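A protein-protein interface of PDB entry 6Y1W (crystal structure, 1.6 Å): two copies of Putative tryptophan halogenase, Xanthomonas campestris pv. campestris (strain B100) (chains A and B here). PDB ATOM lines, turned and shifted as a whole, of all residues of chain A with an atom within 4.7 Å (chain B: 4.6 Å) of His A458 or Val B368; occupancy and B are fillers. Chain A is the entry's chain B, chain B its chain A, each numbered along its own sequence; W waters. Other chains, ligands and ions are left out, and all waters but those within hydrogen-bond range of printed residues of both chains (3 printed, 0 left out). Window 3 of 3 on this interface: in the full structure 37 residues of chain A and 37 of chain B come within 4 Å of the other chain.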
ATOM      1  N   GLN A 428     -18.076   2.904 -18.414  1.00  0.00           N
ATOM      2  CA  GLN A 428     -18.394   4.248 -18.894  1.00  0.00           C
ATOM      3  C   GLN A 428     -19.883   4.418 -19.129  1.00  0.00           C
ATOM      4  O   GLN A 428     -20.466   5.426 -18.729  1.00  0.00           O
ATOM      5  CB  GLN A 428     -17.649   4.561 -20.194  1.00  0.00           C
ATOM      6  CG  GLN A 428     -18.192   5.807 -20.951  1.00  0.00           C
ATOM      7  CD  GLN A 428     -17.914   7.116 -20.226  1.00  0.00           C
ATOM      8  OE1 GLN A 428     -18.611   8.116 -20.428  1.00  0.00           O
ATOM      9  NE2 GLN A 428     -16.891   7.121 -19.396  1.00  0.00           N
ATOM     10  N   SER A 429     -20.523   3.461 -19.818  1.00  0.00           N
ATOM     11  CA  SER A 429     -21.882   3.711 -20.287  1.00  0.00           C
ATOM     12  C   SER A 429     -22.852   2.561 -20.039  1.00  0.00           C
ATOM     13  O   SER A 429     -23.991   2.620 -20.527  1.00  0.00           O
ATOM     14  CB  SER A 429     -21.872   4.074 -21.782  1.00  0.00           C
ATOM     15  OG  SER A 429     -21.244   3.081 -22.575  1.00  0.00           O
ATOM     16  N   GLY A 430     -22.446   1.533 -19.288  1.00  0.00           N
ATOM     17  CA  GLY A 430     -23.354   0.455 -18.961  1.00  0.00           C
ATOM     18  C   GLY A 430     -23.641  -0.473 -20.103  1.00  0.00           C
ATOM     19  O   GLY A 430     -24.569  -1.267 -20.003  1.00  0.00           O
ATOM     20  N   PRO A 456     -21.471   1.386 -13.699  1.00  0.00           N
ATOM     21  CA  PRO A 456     -21.521   2.283 -14.862  1.00  0.00           C
ATOM     22  C   PRO A 456     -21.632   3.740 -14.413  1.00  0.00           C
ATOM     23  O   PRO A 456     -22.427   4.067 -13.532  1.00  0.00           O
ATOM     24  CB  PRO A 456     -22.785   1.822 -15.609  1.00  0.00           C
ATOM     25  CG  PRO A 456     -22.875   0.362 -15.244  1.00  0.00           C
ATOM     26  CD  PRO A 456     -22.462   0.302 -13.782  1.00  0.00           C
ATOM     27  N   ARG A 457     -20.851   4.600 -15.046  1.00  0.00           N
ATOM     28  CA  ARG A 457     -20.874   6.035 -14.755  1.00  0.00           C
ATOM     29  C   ARG A 457     -22.089   6.722 -15.361  1.00  0.00           C
ATOM     30  O   ARG A 457     -22.497   7.792 -14.862  1.00  0.00           O
ATOM     31  CB  ARG A 457     -19.601   6.689 -15.297  1.00  0.00           C
ATOM     32  CG  ARG A 457     -18.300   6.232 -14.628  1.00  0.00           C
ATOM     33  CD  ARG A 457     -17.175   7.165 -15.010  1.00  0.00           C
ATOM     34  NE  ARG A 457     -16.043   6.440 -15.578  1.00  0.00           N
ATOM     35  CZ  ARG A 457     -14.939   6.131 -14.905  1.00  0.00           C
ATOM     36  NH1 ARG A 457     -14.809   6.486 -13.636  1.00  0.00           N
ATOM     37  NH2 ARG A 457     -13.961   5.469 -15.508  1.00  0.00           N
ATOM     38  N   HIS A 458     -22.662   6.136 -16.419  1.00  0.00           N
ATOM     39  CA  HIS A 458     -23.850   6.650 -17.098  1.00  0.00           C
ATOM     40  C   HIS A 458     -24.688   5.473 -17.550  1.00  0.00           C
ATOM     41  O   HIS A 458     -24.190   4.351 -17.685  1.00  0.00           O
ATOM     42  CB  HIS A 458     -23.499   7.479 -18.327  1.00  0.00           C
ATOM     43  CG  HIS A 458     -22.531   8.573 -18.023  1.00  0.00           C
ATOM     44  ND1 HIS A 458     -22.933   9.775 -17.484  1.00  0.00           N
ATOM     45  CD2 HIS A 458     -21.182   8.613 -18.089  1.00  0.00           C
ATOM     46  CE1 HIS A 458     -21.868  10.525 -17.261  1.00  0.00           C
ATOM     47  NE2 HIS A 458     -20.793   9.845 -17.627  1.00  0.00           N
ATOM     48  N   HIS A 459     -25.967   5.738 -17.800  1.00  0.00           N
ATOM     49  CA  HIS A 459     -26.816   4.735 -18.411  1.00  0.00           C
ATOM     50  C   HIS A 459     -27.413   5.349 -19.674  1.00  0.00           C
ATOM     51  O   HIS A 459     -27.239   6.530 -19.960  1.00  0.00           O
ATOM     52  CB  HIS A 459     -27.929   4.255 -17.458  1.00  0.00           C
ATOM     53  CG  HIS A 459     -28.756   5.368 -16.924  1.00  0.00           C
ATOM     54  ND1 HIS A 459     -28.592   5.887 -15.652  1.00  0.00           N
ATOM     55  CD2 HIS A 459     -29.753   6.081 -17.499  1.00  0.00           C
ATOM     56  CE1 HIS A 459     -29.442   6.885 -15.481  1.00  0.00           C
ATOM     57  NE2 HIS A 459     -30.152   7.029 -16.588  1.00  0.00           N
ATOM     58  N   HIS A 460     -28.079   4.515 -20.422  1.00  0.00           N
ATOM     59  CA  HIS A 460     -28.613   4.936 -21.703  1.00  0.00           C
ATOM     60  C   HIS A 460     -29.692   6.007 -21.541  1.00  0.00           C
ATOM     61  O   HIS A 460     -30.631   5.831 -20.738  1.00  0.00           O
ATOM     62  CB  HIS A 460     -29.182   3.730 -22.432  1.00  0.00           C
ATOM     63  CG  HIS A 460     -29.419   3.967 -23.889  1.00  0.00           C
ATOM     64  ND1 HIS A 460     -30.356   4.869 -24.354  1.00  0.00           N
ATOM     65  CD2 HIS A 460     -28.847   3.407 -24.988  1.00  0.00           C
ATOM     66  CE1 HIS A 460     -30.350   4.857 -25.680  1.00  0.00           C
ATOM     67  NE2 HIS A 460     -29.461   3.968 -26.089  1.00  0.00           N
ATOM     68  N   ARG B  14     -20.611  18.661 -20.774  1.00  0.00           N
ATOM     69  CA  ARG B  14     -20.488  17.495 -21.622  1.00  0.00           C
ATOM     70  C   ARG B  14     -21.836  16.861 -21.974  1.00  0.00           C
ATOM     71  O   ARG B  14     -21.874  16.043 -22.893  1.00  0.00           O
ATOM     72  CB  ARG B  14     -19.598  16.447 -20.945  1.00  0.00           C
ATOM     73  CG  ARG B  14     -18.151  16.885 -20.675  1.00  0.00           C
ATOM     74  CD  ARG B  14     -17.343  15.740 -20.068  1.00  0.00           C
ATOM     75  NE  ARG B  14     -17.146  14.613 -20.989  1.00  0.00           N
ATOM     76  CZ  ARG B  14     -16.930  13.358 -20.594  1.00  0.00           C
ATOM     77  NH1 ARG B  14     -16.893  13.071 -19.296  1.00  0.00           N
ATOM     78  NH2 ARG B  14     -16.752  12.381 -21.488  1.00  0.00           N
ATOM     79  N   LEU B  15     -22.928  17.187 -21.281  1.00  0.00           N
ATOM     80  CA  LEU B  15     -24.184  16.488 -21.549  1.00  0.00           C
ATOM     81  C   LEU B  15     -24.680  16.790 -22.961  1.00  0.00           C
ATOM     82  O   LEU B  15     -24.700  17.945 -23.386  1.00  0.00           O
ATOM     83  CB  LEU B  15     -25.244  16.884 -20.530  1.00  0.00           C
ATOM     84  CG  LEU B  15     -24.960  16.341 -19.142  1.00  0.00           C
ATOM     85  CD1 LEU B  15     -25.847  17.063 -18.122  1.00  0.00           C
ATOM     86  CD2 LEU B  15     -25.183  14.835 -19.100  1.00  0.00           C
ATOM     87  N   VAL B  16     -25.083  15.748 -23.694  1.00  0.00           N
ATOM     88  CA  VAL B  16     -25.553  15.913 -25.066  1.00  0.00           C
ATOM     89  C   VAL B  16     -27.044  16.227 -25.027  1.00  0.00           C
ATOM     90  O   VAL B  16     -27.854  15.363 -24.689  1.00  0.00           O
ATOM     91  CB  VAL B  16     -25.267  14.662 -25.904  1.00  0.00           C
ATOM     92  CG1 VAL B  16     -25.858  14.852 -27.286  1.00  0.00           C
ATOM     93  CG2 VAL B  16     -23.718  14.447 -25.972  1.00  0.00           C
ATOM     94  N   PRO B 366     -25.093   8.889 -26.618  1.00  0.00           N
ATOM     95  CA  PRO B 366     -24.313   9.410 -25.484  1.00  0.00           C
ATOM     96  C   PRO B 366     -25.189  10.225 -24.538  1.00  0.00           C
ATOM     97  O   PRO B 366     -25.995  11.061 -24.971  1.00  0.00           O
ATOM     98  CB  PRO B 366     -23.263  10.311 -26.155  1.00  0.00           C
ATOM     99  CG  PRO B 366     -23.962  10.759 -27.480  1.00  0.00           C
ATOM    100  CD  PRO B 366     -24.688   9.489 -27.908  1.00  0.00           C
ATOM    101  N   GLN B 367     -25.039   9.956 -23.238  1.00  0.00           N
ATOM    102  CA  GLN B 367     -25.250  11.027 -22.258  1.00  0.00           C
ATOM    103  C   GLN B 367     -24.121  12.039 -22.355  1.00  0.00           C
ATOM    104  O   GLN B 367     -24.353  13.255 -22.418  1.00  0.00           O
ATOM    105  CB  GLN B 367     -25.302  10.473 -20.835  1.00  0.00           C
ATOM    106  CG  GLN B 367     -26.345   9.458 -20.584  1.00  0.00           C
ATOM    107  CD  GLN B 367     -27.673  10.061 -20.159  1.00  0.00           C
ATOM    108  OE1 GLN B 367     -27.909  11.301 -20.287  1.00  0.00           O
ATOM    109  NE2 GLN B 367     -28.566   9.196 -19.672  1.00  0.00           N
ATOM    110  N   VAL B 368     -22.888  11.558 -22.310  1.00  0.00           N
ATOM    111  CA  VAL B 368     -21.692  12.348 -22.580  1.00  0.00           C
ATOM    112  C   VAL B 368     -20.901  11.557 -23.606  1.00  0.00           C
ATOM    113  O   VAL B 368     -21.018  10.331 -23.665  1.00  0.00           O
ATOM    114  CB  VAL B 368     -20.822  12.614 -21.317  1.00  0.00           C
ATOM    115  CG1 VAL B 368     -21.620  13.363 -20.237  1.00  0.00           C
ATOM    116  CG2 VAL B 368     -20.217  11.293 -20.774  1.00  0.00           C
ATOM    117  N   ILE B 369     -20.173  12.259 -24.465  1.00  0.00           N
ATOM    118  CA  ILE B 369     -19.386  11.581 -25.498  1.00  0.00           C
ATOM    119  C   ILE B 369     -18.096  11.097 -24.858  1.00  0.00           C
ATOM    120  O   ILE B 369     -17.442  11.845 -24.126  1.00  0.00           O
ATOM    121  CB  ILE B 369     -19.131  12.513 -26.693  1.00  0.00           C
ATOM    122  CG1 ILE B 369     -20.473  12.833 -27.366  1.00  0.00           C
ATOM    123  CG2 ILE B 369     -18.220  11.832 -27.732  1.00  0.00           C
ATOM    124  CD1 ILE B 369     -20.429  14.015 -28.303  1.00  0.00           C
ATOM    125  N   ASP B 370     -17.755   9.829 -25.085  1.00  0.00           N
ATOM    126  CA  ASP B 370     -16.561   9.226 -24.475  1.00  0.00           C
ATOM    127  C   ASP B 370     -15.781   8.420 -25.505  1.00  0.00           C
ATOM    128  O   ASP B 370     -16.391   7.726 -26.329  1.00  0.00           O
ATOM    129  CB  ASP B 370     -16.943   8.294 -23.332  1.00  0.00           C
ATOM    130  CG  ASP B 370     -15.738   7.871 -22.520  1.00  0.00           C
ATOM    131  OD1 ASP B 370     -15.376   8.645 -21.597  1.00  0.00           O
ATOM    132  OD2 ASP B 370     -15.141   6.795 -22.808  1.00  0.00           O
HETATM  133  O   HOH W   1     -20.497   7.803 -22.647  1.00  0.00           O
HETATM  134  O   HOH W   2     -28.941  10.148 -16.919  1.00  0.00           O
HETATM  135  O   HOH W   3     -26.724   8.479 -16.962  1.00  0.00           O
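The backbone carbonyl oxygen (O) of His A459 is in hydrogen-bond range of the side-chain amide nitrogen (NE2) of Gln B367, 3.0 Å away. OD1 of Asp B370 sits at hydrogen-bond distance from NE2 of Gln A428.
Printed residues of chain A that touch a printed residue of chain B: Gln A428, His A458, His A459 and His A460. Among the printed residues, 5 pairs touch across the chains. Among the printed residues, no Asp or Glu carboxylate lies within 4 Å of a Lys or Arg side-chain nitrogen of the other chain.
The side-chain carboxylate (OD1) of Asp B370 lies within salt-bridge range of the guanidinium group (NH2) of Arg B14, at 3.98 Å. The backbone NH of Val B16 sits at hydrogen-bond distance from the backbone carbonyl oxygen of Gln B367 (2.9 Å). The backbone carbonyl oxygen of Gln A428 lies within hydrogen-bond range of the backbone NH of His A458.
Of chain B, only Val B368 comes within 4 Å of His A458. Printed residues of chain A within 4 Å of Val B368: Gln A428 (3.6 Å) and His A458 (3.5 Å). Printed residues of chain B within 4 Å of His A460: Gln B367 (3.9 Å). Printed residues of chain A within 4 Å of Gln B367: His A459 and His A460. Leu B15 touches none of the printed residues of chain A. Pro A456 touches none of the printed residues of chain B. The nearest residue of chain B that does not touch His A458 is Gln B367 (4.1 Å). The nearest printed residue of chain A that does not touch Val B368 is Ser A429 (6.6 Å).
No position is printed for both chains. Of the 5 pairs that touch across the chains among the printed residues, none has its exchanged pair printed and touching as well.
Water W1 bridges O of Val B368 (2.8 Å) and OE1 of Gln A428 (2.9 Å). Water W2 lies within hydrogen-bond range of the side-chain amide nitrogen (NE2) of Gln B367 (2.9 Å) and a ring nitrogen (NE2) of His A459 (3.4 Å). Water W3 bridges the backbone NH (N) of His A459 and the side-chain amide nitrogen (NE2) of Gln B367.
Among the printed residues, pairs that only touch across the chains: His A458 with Val B368, Gln A428 with Val B368 and His A460 with Gln B367.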
